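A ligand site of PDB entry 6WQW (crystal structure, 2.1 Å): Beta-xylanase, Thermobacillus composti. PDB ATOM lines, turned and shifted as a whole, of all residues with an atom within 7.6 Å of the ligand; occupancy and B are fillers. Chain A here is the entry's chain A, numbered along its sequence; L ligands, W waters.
Residues that only touch the ligand: Trp 297, Gln 208 and Trp 83.
Hydrophobic or aromatic side chains within 4 Å of the ligand: His 79, Trp 83, His 210, Trp 289 and Trp 297.
Within 4 Å of the ligand: Lys 46, His 79, Trp 83, Asn 131, Glu 132, Gln 208, His 210, Glu 239, Trp 289 and Trp 297.
Water W2 lies within hydrogen-bond range of an oxygen (O2) of the ligand, the indole nitrogen (NE1) of Trp 289 and the side-chain carboxylate (OE2) of Glu 42.
The indole nitrogen (NE1) of Trp 297 sits at hydrogen-bond distance from the side-chain carboxylate (OD2) of Asp 241, 2.8 Å away.
OE1 of Gln 208 lies close to NE2 of His 210.
The side-chain amide nitrogen (ND2) of Asn 175 lies close to the side-chain amide nitrogen (NE2) of Gln 208 (3.3 Å).
ND2 of Asn 131 sits close to NE1 of Trp 83 (3.4 Å).
The backbone carbonyl oxygen (O) of Glu 42 is in hydrogen-bond range of the side-chain amino group (NZ) of Lys 46 (2.9 Å).
OE1 of Glu 132 is in hydrogen-bond range of NE1 of Trp 83 (2.8 Å).
OE2 of Glu 239 is in hydrogen-bond range of ND2 of Asn 175, at 2.9 Å.
The side-chain carboxylate (OE2) of Glu 132 is in hydrogen-bond range of the side-chain amide nitrogen (NE2) of Gln 208 (2.9 Å).
O3 of the ligand is in hydrogen-bond range of NZ of Lys 46 (3.0 Å).
A ring nitrogen (NE2) of His 79 lies within hydrogen-bond range of an oxygen (O3) of the ligand, 2.8 Å away.
The side-chain carboxylate of Glu 132 lies close to an oxygen (O4) of the ligand, 3.5 Å away.
The side-chain amide nitrogen (ND2) of Asn 131 sits at hydrogen-bond distance from an oxygen (O4) of the ligand (2.5 Å).
O1 of the ligand lies within hydrogen-bond range of NE1 of Trp 289 (3.4 Å).
O4 of the ligand lies close to OE2 of Glu 239, at 3.4 Å.
A ring nitrogen (NE2) of His 210 lies within hydrogen-bond range of an oxygen (O5) of the ligand (3.2 Å).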
ATOM      1  N   ALA A  41      13.481  35.812  19.806  1.00  0.00           N
ATOM      2  CA  ALA A  41      13.506  36.916  20.761  1.00  0.00           C
ATOM      3  C   ALA A  41      13.764  36.376  22.167  1.00  0.00           C
ATOM      4  O   ALA A  41      13.042  35.505  22.643  1.00  0.00           O
ATOM      5  CB  ALA A  41      12.195  37.689  20.714  1.00  0.00           C
ATOM      6  N   GLU A  42      14.800  36.908  22.815  1.00  0.00           N
ATOM      7  CA  GLU A  42      15.215  36.372  24.112  1.00  0.00           C
ATOM      8  C   GLU A  42      14.178  36.671  25.191  1.00  0.00           C
ATOM      9  O   GLU A  42      13.823  35.789  25.989  1.00  0.00           O
ATOM     10  CB  GLU A  42      16.577  36.941  24.505  1.00  0.00           C
ATOM     11  CG  GLU A  42      17.055  36.504  25.885  1.00  0.00           C
ATOM     12  CD  GLU A  42      18.352  37.165  26.288  1.00  0.00           C
ATOM     13  OE1 GLU A  42      19.267  37.229  25.441  1.00  0.00           O
ATOM     14  OE2 GLU A  42      18.456  37.617  27.451  1.00  0.00           O
ATOM     15  N   ASN A  43      13.685  37.912  25.240  1.00  0.00           N
ATOM     16  CA  ASN A  43      12.721  38.313  26.256  1.00  0.00           C
ATOM     17  C   ASN A  43      11.566  39.138  25.716  1.00  0.00           C
ATOM     18  O   ASN A  43      10.556  39.292  26.416  1.00  0.00           O
ATOM     19  CB  ASN A  43      13.404  39.131  27.363  1.00  0.00           C
ATOM     20  CG  ASN A  43      14.617  38.432  27.948  1.00  0.00           C
ATOM     21  OD1 ASN A  43      14.505  37.331  28.493  1.00  0.00           O
ATOM     22  ND2 ASN A  43      15.780  39.067  27.836  1.00  0.00           N
ATOM     23  N   LYS A  46       7.897  37.719  25.528  1.00  0.00           N
ATOM     24  CA  LYS A  46       7.379  37.106  26.729  1.00  0.00           C
ATOM     25  C   LYS A  46       6.146  37.862  27.227  1.00  0.00           C
ATOM     26  O   LYS A  46       5.914  39.008  26.833  1.00  0.00           O
ATOM     27  CB  LYS A  46       8.467  37.064  27.801  1.00  0.00           C
ATOM     28  CG  LYS A  46       9.658  36.208  27.390  1.00  0.00           C
ATOM     29  CD  LYS A  46      10.641  36.012  28.531  1.00  0.00           C
ATOM     30  CE  LYS A  46      11.650  34.947  28.177  1.00  0.00           C
ATOM     31  NZ  LYS A  46      13.013  35.244  28.713  1.00  0.00           N
ATOM     32  N   HIS A  79       8.670  32.905  21.114  1.00  0.00           N
ATOM     33  CA  HIS A  79       8.983  32.523  22.486  1.00  0.00           C
ATOM     34  C   HIS A  79       8.696  33.697  23.403  1.00  0.00           C
ATOM     35  O   HIS A  79       9.320  34.752  23.255  1.00  0.00           O
ATOM     36  CB  HIS A  79      10.449  32.094  22.597  1.00  0.00           C
ATOM     37  CG  HIS A  79      10.906  31.844  24.004  1.00  0.00           C
ATOM     38  ND1 HIS A  79      10.883  30.583  24.579  1.00  0.00           N
ATOM     39  CD2 HIS A  79      11.416  32.671  24.945  1.00  0.00           C
ATOM     40  CE1 HIS A  79      11.337  30.656  25.811  1.00  0.00           C
ATOM     41  NE2 HIS A  79      11.669  31.917  26.066  1.00  0.00           N
ATOM     42  N   THR A  80       7.753  33.545  24.327  1.00  0.00           N
ATOM     43  CA  THR A  80       6.935  32.340  24.507  1.00  0.00           C
ATOM     44  C   THR A  80       5.541  32.795  24.942  1.00  0.00           C
ATOM     45  O   THR A  80       5.387  33.882  25.497  1.00  0.00           O
ATOM     46  CB  THR A  80       7.536  31.375  25.546  1.00  0.00           C
ATOM     47  OG1 THR A  80       6.601  30.339  25.846  1.00  0.00           O
ATOM     48  CG2 THR A  80       7.888  32.126  26.820  1.00  0.00           C
ATOM     49  N   TRP A  83       4.217  31.010  30.321  1.00  0.00           N
ATOM     50  CA  TRP A  83       5.387  30.713  31.142  1.00  0.00           C
ATOM     51  C   TRP A  83       5.033  30.943  32.599  1.00  0.00           C
ATOM     52  O   TRP A  83       4.501  31.996  32.953  1.00  0.00           O
ATOM     53  CB  TRP A  83       6.573  31.601  30.731  1.00  0.00           C
ATOM     54  CG  TRP A  83       7.894  31.203  31.340  1.00  0.00           C
ATOM     55  CD1 TRP A  83       8.186  30.011  31.920  1.00  0.00           C
ATOM     56  CD2 TRP A  83       9.079  32.005  31.434  1.00  0.00           C
ATOM     57  NE1 TRP A  83       9.484  30.005  32.377  1.00  0.00           N
ATOM     58  CE2 TRP A  83      10.055  31.220  32.092  1.00  0.00           C
ATOM     59  CE3 TRP A  83       9.425  33.304  31.040  1.00  0.00           C
ATOM     60  CZ2 TRP A  83      11.341  31.684  32.350  1.00  0.00           C
ATOM     61  CZ3 TRP A  83      10.702  33.762  31.308  1.00  0.00           C
ATOM     62  CH2 TRP A  83      11.646  32.963  31.953  1.00  0.00           C
ATOM     63  N   ASP A 128       6.851  28.469  21.071  1.00  0.00           N
ATOM     64  CA  ASP A 128       6.883  27.832  22.378  1.00  0.00           C
ATOM     65  C   ASP A 128       5.597  28.211  23.096  1.00  0.00           C
ATOM     66  O   ASP A 128       5.522  29.279  23.720  1.00  0.00           O
ATOM     67  CB  ASP A 128       8.111  28.273  23.181  1.00  0.00           C
ATOM     68  CG  ASP A 128       9.417  27.820  22.545  1.00  0.00           C
ATOM     69  OD1 ASP A 128       9.411  26.786  21.848  1.00  0.00           O
ATOM     70  OD2 ASP A 128      10.443  28.491  22.766  1.00  0.00           O
ATOM     71  N   ASN A 131       5.867  27.069  28.310  1.00  0.00           N
ATOM     72  CA  ASN A 131       7.283  27.037  28.668  1.00  0.00           C
ATOM     73  C   ASN A 131       7.434  26.599  30.118  1.00  0.00           C
ATOM     74  O   ASN A 131       6.954  27.283  31.018  1.00  0.00           O
ATOM     75  CB  ASN A 131       7.917  28.413  28.451  1.00  0.00           C
ATOM     76  CG  ASN A 131       9.433  28.337  28.337  1.00  0.00           C
ATOM     77  OD1 ASN A 131       9.973  27.576  27.547  1.00  0.00           O
ATOM     78  ND2 ASN A 131      10.124  29.148  29.135  1.00  0.00           N
ATOM     79  N   GLU A 132       8.114  25.473  30.324  1.00  0.00           N
ATOM     80  CA  GLU A 132       8.545  25.018  31.647  1.00  0.00           C
ATOM     81  C   GLU A 132       7.368  24.853  32.607  1.00  0.00           C
ATOM     82  O   GLU A 132       7.244  25.567  33.612  1.00  0.00           O
ATOM     83  CB  GLU A 132       9.599  25.980  32.224  1.00  0.00           C
ATOM     84  CG  GLU A 132      10.595  26.481  31.212  1.00  0.00           C
ATOM     85  CD  GLU A 132      11.672  27.338  31.826  1.00  0.00           C
ATOM     86  OE1 GLU A 132      11.394  27.986  32.861  1.00  0.00           O
ATOM     87  OE2 GLU A 132      12.782  27.347  31.283  1.00  0.00           O
ATOM     88  N   ASN A 175       8.236  23.567  25.576  1.00  0.00           N
ATOM     89  CA  ASN A 175       9.649  23.898  25.770  1.00  0.00           C
ATOM     90  C   ASN A 175      10.011  23.756  27.242  1.00  0.00           C
ATOM     91  O   ASN A 175       9.297  24.277  28.108  1.00  0.00           O
ATOM     92  CB  ASN A 175       9.927  25.319  25.276  1.00  0.00           C
ATOM     93  CG  ASN A 175      11.388  25.574  25.039  1.00  0.00           C
ATOM     94  OD1 ASN A 175      12.053  24.845  24.304  1.00  0.00           O
ATOM     95  ND2 ASN A 175      11.921  26.626  25.654  1.00  0.00           N
ATOM     96  N   ASP A 176      11.108  23.059  27.516  1.00  0.00           N
ATOM     97  CA  ASP A 176      11.537  22.829  28.894  1.00  0.00           C
ATOM     98  C   ASP A 176      13.035  22.573  28.921  1.00  0.00           C
ATOM     99  O   ASP A 176      13.646  22.225  27.906  1.00  0.00           O
ATOM    100  CB  ASP A 176      10.773  21.670  29.530  1.00  0.00           C
ATOM    101  CG  ASP A 176      10.504  21.897  31.001  1.00  0.00           C
ATOM    102  OD1 ASP A 176      11.179  22.743  31.613  1.00  0.00           O
ATOM    103  OD2 ASP A 176       9.595  21.222  31.548  1.00  0.00           O
ATOM    104  N   TYR A 177      13.620  22.730  30.115  1.00  0.00           N
ATOM    105  CA  TYR A 177      15.038  22.532  30.354  1.00  0.00           C
ATOM    106  C   TYR A 177      15.263  21.260  31.180  1.00  0.00           C
ATOM    107  O   TYR A 177      14.313  20.609  31.631  1.00  0.00           O
ATOM    108  CB  TYR A 177      15.654  23.742  31.052  1.00  0.00           C
ATOM    109  CG  TYR A 177      15.052  24.048  32.409  1.00  0.00           C
ATOM    110  CD1 TYR A 177      13.954  24.881  32.530  1.00  0.00           C
ATOM    111  CD2 TYR A 177      15.597  23.499  33.565  1.00  0.00           C
ATOM    112  CE1 TYR A 177      13.407  25.171  33.765  1.00  0.00           C
ATOM    113  CE2 TYR A 177      15.056  23.784  34.812  1.00  0.00           C
ATOM    114  CZ  TYR A 177      13.956  24.617  34.902  1.00  0.00           C
ATOM    115  OH  TYR A 177      13.410  24.904  36.127  1.00  0.00           O
ATOM    116  N   GLN A 208      15.679  22.579  25.471  1.00  0.00           N
ATOM    117  CA  GLN A 208      16.327  23.867  25.711  1.00  0.00           C
ATOM    118  C   GLN A 208      17.844  23.761  25.562  1.00  0.00           C
ATOM    119  O   GLN A 208      18.470  24.710  25.085  1.00  0.00           O
ATOM    120  CB  GLN A 208      15.943  24.409  27.084  1.00  0.00           C
ATOM    121  CG  GLN A 208      14.648  25.209  27.054  1.00  0.00           C
ATOM    122  CD  GLN A 208      14.341  25.880  28.380  1.00  0.00           C
ATOM    123  OE1 GLN A 208      15.249  26.252  29.114  1.00  0.00           O
ATOM    124  NE2 GLN A 208      13.056  26.029  28.683  1.00  0.00           N
ATOM    125  N   HIS A 210      20.375  23.665  27.750  1.00  0.00           N
ATOM    126  CA  HIS A 210      21.228  24.444  28.655  1.00  0.00           C
ATOM    127  C   HIS A 210      22.184  23.485  29.357  1.00  0.00           C
ATOM    128  O   HIS A 210      21.963  23.051  30.485  1.00  0.00           O
ATOM    129  CB  HIS A 210      20.376  25.242  29.634  1.00  0.00           C
ATOM    130  CG  HIS A 210      19.618  26.368  29.000  1.00  0.00           C
ATOM    131  ND1 HIS A 210      20.244  27.404  28.337  1.00  0.00           N
ATOM    132  CD2 HIS A 210      18.286  26.615  28.930  1.00  0.00           C
ATOM    133  CE1 HIS A 210      19.327  28.237  27.886  1.00  0.00           C
ATOM    134  NE2 HIS A 210      18.137  27.784  28.223  1.00  0.00           N
ATOM    135  N   THR A 238      16.289  24.493  21.334  1.00  0.00           N
ATOM    136  CA  THR A 238      15.779  25.856  21.291  1.00  0.00           C
ATOM    137  C   THR A 238      16.685  26.903  21.918  1.00  0.00           C
ATOM    138  O   THR A 238      16.640  28.065  21.510  1.00  0.00           O
ATOM    139  CB  THR A 238      14.401  25.920  21.980  1.00  0.00           C
ATOM    140  OG1 THR A 238      14.521  25.448  23.329  1.00  0.00           O
ATOM    141  CG2 THR A 238      13.393  25.061  21.233  1.00  0.00           C
ATOM    142  N   GLU A 239      17.493  26.540  22.921  1.00  0.00           N
ATOM    143  CA  GLU A 239      18.251  27.538  23.679  1.00  0.00           C
ATOM    144  C   GLU A 239      19.640  27.012  24.027  1.00  0.00           C
ATOM    145  O   GLU A 239      20.120  27.158  25.154  1.00  0.00           O
ATOM    146  CB  GLU A 239      17.504  27.929  24.962  1.00  0.00           C
ATOM    147  CG  GLU A 239      15.986  28.059  24.784  1.00  0.00           C
ATOM    148  CD  GLU A 239      15.287  28.475  26.059  1.00  0.00           C
ATOM    149  OE1 GLU A 239      15.987  28.665  27.068  1.00  0.00           O
ATOM    150  OE2 GLU A 239      14.044  28.601  26.031  1.00  0.00           O
ATOM    151  N   ASP A 241      23.328  26.174  24.849  1.00  0.00           N
ATOM    152  CA  ASP A 241      24.623  26.741  25.200  1.00  0.00           C
ATOM    153  C   ASP A 241      25.388  25.730  26.038  1.00  0.00           C
ATOM    154  O   ASP A 241      24.808  24.790  26.594  1.00  0.00           O
ATOM    155  CB  ASP A 241      24.498  28.077  25.933  1.00  0.00           C
ATOM    156  CG  ASP A 241      23.323  28.129  26.887  1.00  0.00           C
ATOM    157  OD1 ASP A 241      22.983  27.075  27.477  1.00  0.00           O
ATOM    158  OD2 ASP A 241      22.741  29.220  27.048  1.00  0.00           O
ATOM    159  N   TRP A 289      21.148  29.964  22.613  1.00  0.00           N
ATOM    160  CA  TRP A 289      20.610  31.050  23.446  1.00  0.00           C
ATOM    161  C   TRP A 289      21.626  32.180  23.513  1.00  0.00           C
ATOM    162  O   TRP A 289      22.236  32.483  24.544  1.00  0.00           O
ATOM    163  CB  TRP A 289      20.232  30.545  24.832  1.00  0.00           C
ATOM    164  CG  TRP A 289      19.128  31.360  25.433  1.00  0.00           C
ATOM    165  CD1 TRP A 289      19.156  32.055  26.603  1.00  0.00           C
ATOM    166  CD2 TRP A 289      17.823  31.582  24.876  1.00  0.00           C
ATOM    167  NE1 TRP A 289      17.965  32.689  26.814  1.00  0.00           N
ATOM    168  CE2 TRP A 289      17.123  32.418  25.768  1.00  0.00           C
ATOM    169  CE3 TRP A 289      17.178  31.142  23.713  1.00  0.00           C
ATOM    170  CZ2 TRP A 289      15.814  32.825  25.532  1.00  0.00           C
ATOM    171  CZ3 TRP A 289      15.875  31.557  23.477  1.00  0.00           C
ATOM    172  CH2 TRP A 289      15.208  32.392  24.385  1.00  0.00           C
ATOM    173  N   TRP A 297      23.101  35.026  28.735  1.00  0.00           N
ATOM    174  CA  TRP A 297      22.340  35.077  29.977  1.00  0.00           C
ATOM    175  C   TRP A 297      23.064  34.382  31.122  1.00  0.00           C
ATOM    176  O   TRP A 297      22.784  34.681  32.286  1.00  0.00           O
ATOM    177  CB  TRP A 297      20.960  34.448  29.770  1.00  0.00           C
ATOM    178  CG  TRP A 297      21.009  32.957  29.681  1.00  0.00           C
ATOM    179  CD1 TRP A 297      21.616  32.216  28.701  1.00  0.00           C
ATOM    180  CD2 TRP A 297      20.450  32.018  30.604  1.00  0.00           C
ATOM    181  NE1 TRP A 297      21.454  30.874  28.959  1.00  0.00           N
ATOM    182  CE2 TRP A 297      20.751  30.729  30.118  1.00  0.00           C
ATOM    183  CE3 TRP A 297      19.736  32.142  31.795  1.00  0.00           C
ATOM    184  CZ2 TRP A 297      20.335  29.574  30.780  1.00  0.00           C
ATOM    185  CZ3 TRP A 297      19.328  30.994  32.447  1.00  0.00           C
ATOM    186  CH2 TRP A 297      19.628  29.729  31.945  1.00  0.00           C
ATOM    187  N   LEU A 298      23.969  33.456  30.813  1.00  0.00           N
ATOM    188  CA  LEU A 298      24.742  32.777  31.849  1.00  0.00           C
ATOM    189  C   LEU A 298      25.685  33.714  32.579  1.00  0.00           C
ATOM    190  O   LEU A 298      26.178  33.368  33.661  1.00  0.00           O
ATOM    191  CB  LEU A 298      25.527  31.613  31.230  1.00  0.00           C
ATOM    192  CG  LEU A 298      24.676  30.577  30.506  1.00  0.00           C
ATOM    193  CD1 LEU A 298      25.532  29.635  29.685  1.00  0.00           C
ATOM    194  CD2 LEU A 298      23.826  29.802  31.500  1.00  0.00           C
ATOM    195  N   PHE A 301      23.103  34.615  35.456  1.00  0.00           N
ATOM    196  CA  PHE A 301      22.404  33.551  36.154  1.00  0.00           C
ATOM    197  C   PHE A 301      23.280  32.309  36.096  1.00  0.00           C
ATOM    198  O   PHE A 301      23.817  31.989  35.012  1.00  0.00           O
ATOM    199  CB  PHE A 301      21.021  33.265  35.550  1.00  0.00           C
ATOM    200  CG  PHE A 301      20.337  32.062  36.115  1.00  0.00           C
ATOM    201  CD1 PHE A 301      20.529  30.802  35.553  1.00  0.00           C
ATOM    202  CD2 PHE A 301      19.495  32.165  37.207  1.00  0.00           C
ATOM    203  CE1 PHE A 301      19.905  29.687  36.067  1.00  0.00           C
ATOM    204  CE2 PHE A 301      18.862  31.058  37.729  1.00  0.00           C
ATOM    205  CZ  PHE A 301      19.067  29.814  37.165  1.00  0.00           C
HETATM  206  O1  LIG L   1      17.595  31.272  29.834  1.00  0.00           O
HETATM  207  C1  LIG L   1      16.306  31.016  30.183  1.00  0.00           C
HETATM  208  C2  LIG L   1      15.406  32.001  29.411  1.00  0.00           C
HETATM  209  C3  LIG L   1      13.990  31.571  29.228  1.00  0.00           C
HETATM  210  C4  LIG L   1      13.870  30.129  28.861  1.00  0.00           C
HETATM  211  C5  LIG L   1      14.605  29.260  29.880  1.00  0.00           C
HETATM  212  O2  LIG L   1      15.402  33.251  30.132  1.00  0.00           O
HETATM  213  O3  LIG L   1      13.418  32.355  28.150  1.00  0.00           O
HETATM  214  O4  LIG L   1      12.492  29.757  28.816  1.00  0.00           O
HETATM  215  O5  LIG L   1      16.044  29.568  29.908  1.00  0.00           O
HETATM  216  O   HOH W   1      15.399  34.357  32.648  1.00  0.00           O
HETATM  217  O   HOH W   2      17.473  34.789  28.801  1.00  0.00           O
